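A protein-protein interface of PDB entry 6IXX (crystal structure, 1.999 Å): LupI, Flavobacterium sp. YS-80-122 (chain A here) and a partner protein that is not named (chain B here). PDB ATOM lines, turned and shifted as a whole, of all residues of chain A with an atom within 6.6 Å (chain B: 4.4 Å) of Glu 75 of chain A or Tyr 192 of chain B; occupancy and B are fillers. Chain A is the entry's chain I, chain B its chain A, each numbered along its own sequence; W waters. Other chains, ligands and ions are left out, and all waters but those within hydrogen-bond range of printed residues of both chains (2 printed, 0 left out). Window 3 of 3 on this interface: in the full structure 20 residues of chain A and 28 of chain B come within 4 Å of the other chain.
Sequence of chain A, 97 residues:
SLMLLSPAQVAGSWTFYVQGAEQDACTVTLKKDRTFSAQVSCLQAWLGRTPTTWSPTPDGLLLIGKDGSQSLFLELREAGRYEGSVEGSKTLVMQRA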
ATOM      1  N   ASP A  59     -13.750  -0.095  13.690  1.00  0.00           N
ATOM      2  CA  ASP A  59     -13.626  -0.938  14.869  1.00  0.00           C
ATOM      3  C   ASP A  59     -14.768  -1.937  15.019  1.00  0.00           C
ATOM      4  O   ASP A  59     -14.794  -2.688  16.001  1.00  0.00           O
ATOM      5  CB  ASP A  59     -13.546  -0.068  16.131  1.00  0.00           C
ATOM      6  CG  ASP A  59     -14.826   0.752  16.378  1.00  0.00           C
ATOM      7  OD1 ASP A  59     -15.430   1.228  15.391  1.00  0.00           O
ATOM      8  OD2 ASP A  59     -15.226   0.928  17.560  1.00  0.00           O
ATOM      9  N   GLY A  60     -15.719  -1.965  14.089  1.00  0.00           N
ATOM     10  CA  GLY A  60     -16.829  -2.877  14.272  1.00  0.00           C
ATOM     11  C   GLY A  60     -17.832  -2.825  13.143  1.00  0.00           C
ATOM     12  O   GLY A  60     -17.455  -2.701  11.974  1.00  0.00           O
ATOM     13  N   LEU A  61     -19.115  -2.904  13.489  1.00  0.00           N
ATOM     14  CA  LEU A  61     -20.168  -2.984  12.490  1.00  0.00           C
ATOM     15  C   LEU A  61     -21.477  -2.528  13.113  1.00  0.00           C
ATOM     16  O   LEU A  61     -21.785  -2.881  14.251  1.00  0.00           O
ATOM     17  CB  LEU A  61     -20.320  -4.408  11.957  1.00  0.00           C
ATOM     18  CG  LEU A  61     -21.318  -4.657  10.822  1.00  0.00           C
ATOM     19  CD1 LEU A  61     -20.604  -4.621   9.507  1.00  0.00           C
ATOM     20  CD2 LEU A  61     -21.991  -6.000  11.006  1.00  0.00           C
ATOM     21  N   PHE A  73     -24.635  -1.746  17.718  1.00  0.00           N
ATOM     22  CA  PHE A  73     -23.214  -1.790  17.409  1.00  0.00           C
ATOM     23  C   PHE A  73     -22.622  -3.110  17.885  1.00  0.00           C
ATOM     24  O   PHE A  73     -22.973  -3.609  18.957  1.00  0.00           O
ATOM     25  CB  PHE A  73     -22.452  -0.633  18.064  1.00  0.00           C
ATOM     26  CG  PHE A  73     -20.956  -0.683  17.824  1.00  0.00           C
ATOM     27  CD1 PHE A  73     -20.439  -0.421  16.564  1.00  0.00           C
ATOM     28  CD2 PHE A  73     -20.079  -1.023  18.845  1.00  0.00           C
ATOM     29  CE1 PHE A  73     -19.062  -0.477  16.323  1.00  0.00           C
ATOM     30  CE2 PHE A  73     -18.703  -1.080  18.617  1.00  0.00           C
ATOM     31  CZ  PHE A  73     -18.199  -0.809  17.347  1.00  0.00           C
ATOM     32  N   LEU A  74     -21.729  -3.673  17.074  1.00  0.00           N
ATOM     33  CA  LEU A  74     -20.917  -4.817  17.464  1.00  0.00           C
ATOM     34  C   LEU A  74     -19.466  -4.485  17.156  1.00  0.00           C
ATOM     35  O   LEU A  74     -19.160  -3.957  16.083  1.00  0.00           O
ATOM     36  CB  LEU A  74     -21.291  -6.114  16.725  1.00  0.00           C
ATOM     37  CG  LEU A  74     -22.702  -6.696  16.701  1.00  0.00           C
ATOM     38  CD1 LEU A  74     -23.594  -5.854  15.859  1.00  0.00           C
ATOM     39  CD2 LEU A  74     -22.610  -8.081  16.086  1.00  0.00           C
ATOM     40  N   GLU A  75     -18.586  -4.807  18.097  1.00  0.00           N
ATOM     41  CA  GLU A  75     -17.164  -4.513  17.984  1.00  0.00           C
ATOM     42  C   GLU A  75     -16.437  -5.697  17.363  1.00  0.00           C
ATOM     43  O   GLU A  75     -16.680  -6.850  17.736  1.00  0.00           O
ATOM     44  CB  GLU A  75     -16.577  -4.202  19.369  1.00  0.00           C
ATOM     45  CG  GLU A  75     -15.078  -3.844  19.386  1.00  0.00           C
ATOM     46  CD  GLU A  75     -14.564  -3.542  20.804  1.00  0.00           C
ATOM     47  OE1 GLU A  75     -14.184  -4.502  21.505  1.00  0.00           O
ATOM     48  OE2 GLU A  75     -14.553  -2.355  21.222  1.00  0.00           O
ATOM     49  N   LEU A  76     -15.543  -5.404  16.418  1.00  0.00           N
ATOM     50  CA  LEU A  76     -14.740  -6.451  15.789  1.00  0.00           C
ATOM     51  C   LEU A  76     -13.766  -7.016  16.812  1.00  0.00           C
ATOM     52  O   LEU A  76     -12.912  -6.290  17.329  1.00  0.00           O
ATOM     53  CB  LEU A  76     -13.988  -5.898  14.579  1.00  0.00           C
ATOM     54  CG  LEU A  76     -13.076  -6.842  13.774  1.00  0.00           C
ATOM     55  CD1 LEU A  76     -13.838  -7.993  13.121  1.00  0.00           C
ATOM     56  CD2 LEU A  76     -12.324  -6.048  12.731  1.00  0.00           C
ATOM     57  N   ARG A  77     -13.901  -8.303  17.120  1.00  0.00           N
ATOM     58  CA  ARG A  77     -13.094  -8.897  18.176  1.00  0.00           C
ATOM     59  C   ARG A  77     -11.834  -9.559  17.644  1.00  0.00           C
ATOM     60  O   ARG A  77     -10.809  -9.578  18.334  1.00  0.00           O
ATOM     61  CB  ARG A  77     -13.925  -9.915  18.966  1.00  0.00           C
ATOM     62  CG  ARG A  77     -14.953  -9.270  19.884  1.00  0.00           C
ATOM     63  CD  ARG A  77     -14.476  -9.182  21.345  1.00  0.00           C
ATOM     64  NE  ARG A  77     -13.019  -9.108  21.442  1.00  0.00           N
ATOM     65  CZ  ARG A  77     -12.293  -8.017  21.201  1.00  0.00           C
ATOM     66  NH1 ARG A  77     -12.887  -6.883  20.847  1.00  0.00           N
ATOM     67  NH2 ARG A  77     -10.968  -8.069  21.304  1.00  0.00           N
ATOM     68  N   GLU A  78     -11.902 -10.082  16.427  1.00  0.00           N
ATOM     69  CA  GLU A  78     -10.826 -10.764  15.721  1.00  0.00           C
ATOM     70  C   GLU A  78     -11.352 -10.964  14.312  1.00  0.00           C
ATOM     71  O   GLU A  78     -12.539 -10.755  14.053  1.00  0.00           O
ATOM     72  CB  GLU A  78     -10.457 -12.098  16.373  1.00  0.00           C
ATOM     73  CG  GLU A  78     -11.452 -13.218  16.067  1.00  0.00           C
ATOM     74  CD  GLU A  78     -11.167 -14.491  16.848  1.00  0.00           C
ATOM     75  OE1 GLU A  78     -11.874 -14.767  17.844  1.00  0.00           O
ATOM     76  OE2 GLU A  78     -10.230 -15.217  16.466  1.00  0.00           O
ATOM     77  N   ARG A  81     -15.057 -12.034  13.314  1.00  0.00           N
ATOM     78  CA  ARG A  81     -15.869 -12.178  14.520  1.00  0.00           C
ATOM     79  C   ARG A  81     -16.185 -10.822  15.131  1.00  0.00           C
ATOM     80  O   ARG A  81     -15.270 -10.078  15.499  1.00  0.00           O
ATOM     81  CB  ARG A  81     -15.173 -13.057  15.560  1.00  0.00           C
ATOM     82  CG  ARG A  81     -15.993 -13.290  16.811  1.00  0.00           C
ATOM     83  CD  ARG A  81     -15.156 -14.062  17.821  1.00  0.00           C
ATOM     84  NE  ARG A  81     -15.827 -14.293  19.097  1.00  0.00           N
ATOM     85  CZ  ARG A  81     -16.359 -15.450  19.470  1.00  0.00           C
ATOM     86  NH1 ARG A  81     -16.336 -16.498  18.651  1.00  0.00           N
ATOM     87  NH2 ARG A  81     -16.923 -15.561  20.665  1.00  0.00           N
ATOM     88  N   TYR A  82     -17.478 -10.530  15.282  1.00  0.00           N
ATOM     89  CA  TYR A  82     -17.963  -9.358  15.995  1.00  0.00           C
ATOM     90  C   TYR A  82     -18.763  -9.808  17.209  1.00  0.00           C
ATOM     91  O   TYR A  82     -19.378 -10.879  17.203  1.00  0.00           O
ATOM     92  CB  TYR A  82     -18.866  -8.465  15.108  1.00  0.00           C
ATOM     93  CG  TYR A  82     -18.261  -8.018  13.791  1.00  0.00           C
ATOM     94  CD1 TYR A  82     -18.322  -8.833  12.657  1.00  0.00           C
ATOM     95  CD2 TYR A  82     -17.645  -6.772  13.670  1.00  0.00           C
ATOM     96  CE1 TYR A  82     -17.782  -8.415  11.441  1.00  0.00           C
ATOM     97  CE2 TYR A  82     -17.102  -6.348  12.470  1.00  0.00           C
ATOM     98  CZ  TYR A  82     -17.166  -7.175  11.357  1.00  0.00           C
ATOM     99  OH  TYR A  82     -16.631  -6.767  10.156  1.00  0.00           O
ATOM    100  N   GLU A  83     -18.772  -8.969  18.246  1.00  0.00           N
ATOM    101  CA  GLU A  83     -19.545  -9.225  19.453  1.00  0.00           C
ATOM    102  C   GLU A  83     -20.298  -7.965  19.864  1.00  0.00           C
ATOM    103  O   GLU A  83     -19.787  -6.847  19.749  1.00  0.00           O
ATOM    104  CB  GLU A  83     -18.647  -9.710  20.596  1.00  0.00           C
ATOM    105  CG  GLU A  83     -17.957 -11.040  20.257  1.00  0.00           C
ATOM    106  CD  GLU A  83     -17.103 -11.586  21.385  1.00  0.00           C
ATOM    107  OE1 GLU A  83     -16.996 -10.918  22.431  1.00  0.00           O
ATOM    108  OE2 GLU A  83     -16.526 -12.683  21.218  1.00  0.00           O
ATOM    109  N   GLY A  84     -21.524  -8.152  20.331  1.00  0.00           N
ATOM    110  CA  GLY A  84     -22.284  -7.059  20.891  1.00  0.00           C
ATOM    111  C   GLY A  84     -23.158  -7.577  22.014  1.00  0.00           C
ATOM    112  O   GLY A  84     -23.223  -8.781  22.275  1.00  0.00           O
ATOM    113  N   ASN B  26     -19.922   3.421  31.131  1.00  0.00           N
ATOM    114  CA  ASN B  26     -19.574   2.110  30.584  1.00  0.00           C
ATOM    115  C   ASN B  26     -18.522   1.403  31.435  1.00  0.00           C
ATOM    116  O   ASN B  26     -17.612   0.752  30.919  1.00  0.00           O
ATOM    117  CB  ASN B  26     -19.121   2.253  29.126  1.00  0.00           C
ATOM    118  CG  ASN B  26     -20.258   2.670  28.231  1.00  0.00           C
ATOM    119  OD1 ASN B  26     -21.401   2.336  28.519  1.00  0.00           O
ATOM    120  ND2 ASN B  26     -19.972   3.420  27.164  1.00  0.00           N
ATOM    121  N   LYS B  28     -16.160   2.700  33.208  1.00  0.00           N
ATOM    122  CA  LYS B  28     -14.895   3.411  33.173  1.00  0.00           C
ATOM    123  C   LYS B  28     -15.051   4.785  33.811  1.00  0.00           C
ATOM    124  O   LYS B  28     -16.156   5.337  33.850  1.00  0.00           O
ATOM    125  CB  LYS B  28     -14.407   3.567  31.723  1.00  0.00           C
ATOM    126  CG  LYS B  28     -14.060   2.242  31.042  1.00  0.00           C
ATOM    127  CD  LYS B  28     -13.796   2.422  29.536  1.00  0.00           C
ATOM    128  CE  LYS B  28     -15.010   2.035  28.713  1.00  0.00           C
ATOM    129  NZ  LYS B  28     -15.265   0.542  28.658  1.00  0.00           N
ATOM    130  N   SER B 191      -9.747  -3.086  22.345  1.00  0.00           N
ATOM    131  CA  SER B 191     -11.192  -3.024  22.528  1.00  0.00           C
ATOM    132  C   SER B 191     -11.552  -1.801  23.366  1.00  0.00           C
ATOM    133  O   SER B 191     -10.777  -1.371  24.229  1.00  0.00           O
ATOM    134  CB  SER B 191     -11.728  -4.304  23.213  1.00  0.00           C
ATOM    135  OG  SER B 191     -13.025  -4.101  23.775  1.00  0.00           O
ATOM    136  N   TYR B 192     -12.753  -1.261  23.124  1.00  0.00           N
ATOM    137  CA  TYR B 192     -13.263  -0.192  23.982  1.00  0.00           C
ATOM    138  C   TYR B 192     -13.420  -0.660  25.427  1.00  0.00           C
ATOM    139  O   TYR B 192     -13.303   0.146  26.358  1.00  0.00           O
ATOM    140  CB  TYR B 192     -14.599   0.321  23.438  1.00  0.00           C
ATOM    141  CG  TYR B 192     -15.318   1.331  24.316  1.00  0.00           C
ATOM    142  CD1 TYR B 192     -14.928   2.664  24.341  1.00  0.00           C
ATOM    143  CD2 TYR B 192     -16.394   0.945  25.116  1.00  0.00           C
ATOM    144  CE1 TYR B 192     -15.595   3.597  25.133  1.00  0.00           C
ATOM    145  CE2 TYR B 192     -17.068   1.859  25.907  1.00  0.00           C
ATOM    146  CZ  TYR B 192     -16.666   3.192  25.910  1.00  0.00           C
ATOM    147  OH  TYR B 192     -17.326   4.114  26.697  1.00  0.00           O
ATOM    148  N   ARG B 193     -13.667  -1.957  25.634  1.00  0.00           N
ATOM    149  CA  ARG B 193     -13.798  -2.493  26.989  1.00  0.00           C
ATOM    150  C   ARG B 193     -12.620  -2.109  27.883  1.00  0.00           C
ATOM    151  O   ARG B 193     -12.790  -1.919  29.096  1.00  0.00           O
ATOM    152  CB  ARG B 193     -13.943  -4.022  26.937  1.00  0.00           C
ATOM    153  CG  ARG B 193     -15.366  -4.514  26.664  1.00  0.00           C
ATOM    154  CD  ARG B 193     -15.421  -6.034  26.513  1.00  0.00           C
ATOM    155  NE  ARG B 193     -14.459  -6.519  25.526  1.00  0.00           N
ATOM    156  CZ  ARG B 193     -14.388  -7.775  25.092  1.00  0.00           C
ATOM    157  NH1 ARG B 193     -15.223  -8.698  25.556  1.00  0.00           N
ATOM    158  NH2 ARG B 193     -13.472  -8.108  24.198  1.00  0.00           N
ATOM    159  N   ASP B 194     -11.421  -2.009  27.315  1.00  0.00           N
ATOM    160  CA  ASP B 194     -10.228  -1.671  28.071  1.00  0.00           C
ATOM    161  C   ASP B 194      -9.819  -0.211  27.909  1.00  0.00           C
ATOM    162  O   ASP B 194      -8.670   0.138  28.216  1.00  0.00           O
ATOM    163  CB  ASP B 194      -9.089  -2.601  27.666  1.00  0.00           C
ATOM    164  CG  ASP B 194      -9.533  -4.049  27.618  1.00  0.00           C
ATOM    165  OD1 ASP B 194     -10.020  -4.551  28.659  1.00  0.00           O
ATOM    166  OD2 ASP B 194      -9.425  -4.670  26.535  1.00  0.00           O
ATOM    167  N   ALA B 195     -10.734   0.656  27.471  1.00  0.00           N
ATOM    168  CA  ALA B 195     -10.398   2.066  27.364  1.00  0.00           C
ATOM    169  C   ALA B 195     -10.100   2.661  28.748  1.00  0.00           C
ATOM    170  O   ALA B 195     -10.491   2.124  29.790  1.00  0.00           O
ATOM    171  CB  ALA B 195     -11.523   2.834  26.673  1.00  0.00           C
ATOM    172  N   GLY B 198     -14.492   6.729  29.826  1.00  0.00           N
ATOM    173  CA  GLY B 198     -15.692   6.392  29.087  1.00  0.00           C
ATOM    174  C   GLY B 198     -15.796   7.135  27.772  1.00  0.00           C
ATOM    175  O   GLY B 198     -16.266   6.585  26.768  1.00  0.00           O
ATOM    176  N   ASP B 200     -13.713   7.960  25.576  1.00  0.00           N
ATOM    177  CA  ASP B 200     -12.835   7.578  24.474  1.00  0.00           C
ATOM    178  C   ASP B 200     -13.687   6.968  23.356  1.00  0.00           C
ATOM    179  O   ASP B 200     -13.730   5.755  23.148  1.00  0.00           O
ATOM    180  CB  ASP B 200     -11.763   6.610  24.961  1.00  0.00           C
ATOM    181  CG  ASP B 200     -10.807   6.196  23.862  1.00  0.00           C
ATOM    182  OD1 ASP B 200     -10.838   6.821  22.785  1.00  0.00           O
ATOM    183  OD2 ASP B 200     -10.006   5.267  24.082  1.00  0.00           O
ATOM    184  N   THR B 201     -14.408   7.844  22.647  1.00  0.00           N
ATOM    185  CA  THR B 201     -15.082   7.457  21.417  1.00  0.00           C
ATOM    186  C   THR B 201     -14.994   8.596  20.409  1.00  0.00           C
ATOM    187  O   THR B 201     -14.609   9.729  20.726  1.00  0.00           O
ATOM    188  CB  THR B 201     -16.568   7.086  21.610  1.00  0.00           C
ATOM    189  OG1 THR B 201     -17.341   8.274  21.828  1.00  0.00           O
ATOM    190  CG2 THR B 201     -16.790   6.081  22.749  1.00  0.00           C
ATOM    191  N   TRP B 210     -12.744   4.163  18.855  1.00  0.00           N
ATOM    192  CA  TRP B 210     -13.976   3.481  19.245  1.00  0.00           C
ATOM    193  C   TRP B 210     -15.228   4.216  18.781  1.00  0.00           C
ATOM    194  O   TRP B 210     -15.320   5.444  18.873  1.00  0.00           O
ATOM    195  CB  TRP B 210     -13.994   3.276  20.761  1.00  0.00           C
ATOM    196  CG  TRP B 210     -12.677   2.739  21.244  1.00  0.00           C
ATOM    197  CD1 TRP B 210     -11.888   3.260  22.231  1.00  0.00           C
ATOM    198  CD2 TRP B 210     -11.976   1.588  20.738  1.00  0.00           C
ATOM    199  NE1 TRP B 210     -10.756   2.501  22.379  1.00  0.00           N
ATOM    200  CE2 TRP B 210     -10.784   1.470  21.475  1.00  0.00           C
ATOM    201  CE3 TRP B 210     -12.242   0.647  19.731  1.00  0.00           C
ATOM    202  CZ2 TRP B 210      -9.853   0.455  21.237  1.00  0.00           C
ATOM    203  CZ3 TRP B 210     -11.314  -0.357  19.493  1.00  0.00           C
ATOM    204  CH2 TRP B 210     -10.137  -0.445  20.246  1.00  0.00           C
ATOM    205  N   ASN B 214     -20.748   3.474  21.168  1.00  0.00           N
ATOM    206  CA  ASN B 214     -20.376   2.940  22.474  1.00  0.00           C
ATOM    207  C   ASN B 214     -20.857   3.832  23.614  1.00  0.00           C
ATOM    208  O   ASN B 214     -21.206   3.337  24.687  1.00  0.00           O
ATOM    209  CB  ASN B 214     -18.859   2.788  22.560  1.00  0.00           C
ATOM    210  CG  ASN B 214     -18.356   1.539  21.879  1.00  0.00           C
ATOM    211  OD1 ASN B 214     -18.703   0.434  22.269  1.00  0.00           O
ATOM    212  ND2 ASN B 214     -17.510   1.713  20.860  1.00  0.00           N
ATOM    213  N   THR B 215     -20.865   5.144  23.416  1.00  0.00           N
ATOM    214  CA  THR B 215     -21.363   6.054  24.429  1.00  0.00           C
ATOM    215  C   THR B 215     -22.782   6.524  24.146  1.00  0.00           C
ATOM    216  O   THR B 215     -23.257   7.444  24.811  1.00  0.00           O
ATOM    217  CB  THR B 215     -20.428   7.253  24.573  1.00  0.00           C
ATOM    218  OG1 THR B 215     -19.999   7.699  23.276  1.00  0.00           O
ATOM    219  CG2 THR B 215     -19.214   6.860  25.419  1.00  0.00           C
HETATM  220  O   HOH W   1     -17.458  -1.865  22.318  1.00  0.00           O
HETATM  221  O   HOH W   2     -15.681  -0.241  19.988  1.00  0.00           O
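N of Tyr 192 of chain B is in hydrogen-bond range of OE2 of Glu 75 of chain A (2.8 Å). The side-chain carboxylate of Glu 75 of chain A is in hydrogen-bond range of the side-chain hydroxyl of Ser 191 of chain B (2.6 Å). The guanidinium group (NE) of Arg 77 of chain A sits close to the guanidinium group (NH2) of Arg 193 of chain B, at 3.0 Å.
The side-chain amide nitrogen of Asn 26 of chain B is in hydrogen-bond range of the side-chain hydroxyl of Tyr 192 of chain B (2.8 Å). The backbone NH of Arg 193 of chain B sits at hydrogen-bond distance from the side-chain hydroxyl of Ser 191 of chain B (2.9 Å). O of Asn 214 of chain B is in hydrogen-bond range of ND2 of Asn 26 of chain B (2.8 Å). N of Glu 75 of chain A lies within hydrogen-bond range of O of Glu 83 of chain A. The side-chain carboxylate of Asp 200 of chain B sits close to the indole nitrogen of Trp 210 of chain B, 3.3 Å away. The side-chain carboxylate (OE1) of Glu 75 of chain A lies within salt-bridge range of the guanidinium group (NH1) of Arg 77 of chain A, 2.8 Å away.
Trp 210 of chain B touches Asp 59 of chain A. CE2 of Phe 73 of chain A touches ND2 of Asn 214 of chain B (3.8 Å). CB of Ser 191 of chain B touches NH1 of Arg 77 of chain A (3.7 Å).
Glu 75 of chain A touches just these residues of chain B: Ser 191 (2.6 Å) and Tyr 192 (2.8 Å). Tyr 192 of chain B touches one residue of chain A. Printed residues of chain B within 4 Å of Arg 77 of chain A: Ser 191 and Arg 193. Printed residues of chain A within 4 Å of Arg 193 of chain B: Arg 77. Of the printed residues of chain A, Trp 210 of chain B touches Asp 59. Printed residues of chain A within 4 Å of Ser 191 of chain B: Glu 75 (2.6 Å) and Arg 77 (3.7 Å). Gly 84 of chain A touches none of the printed residues of chain B. The nearest residue of chain B that does not touch Glu 75 of chain A is Trp 210 of chain B (4.1 Å). The nearest residue of chain A that does not touch Tyr 192 of chain B is Asp 59 of chain A (5.9 Å).
Of the 13 printed residues of chain B, 5 touch a printed residue of chain A. Of the 13 printed residues of chain A, 4 touch a printed residue of chain B.
Water W1 bridges OD1 of Asn 214 of chain B (2.6 Å) and OE2 of Glu 75 of chain A (3.1 Å). Water W2 lies within hydrogen-bond range of the side-chain carboxylate of Glu 75 of chain A (2.7 Å), the side-chain carboxylate of Asp 59 of chain A (2.7 Å) and the side-chain amide nitrogen of Asn 214 of chain B (2.8 Å).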
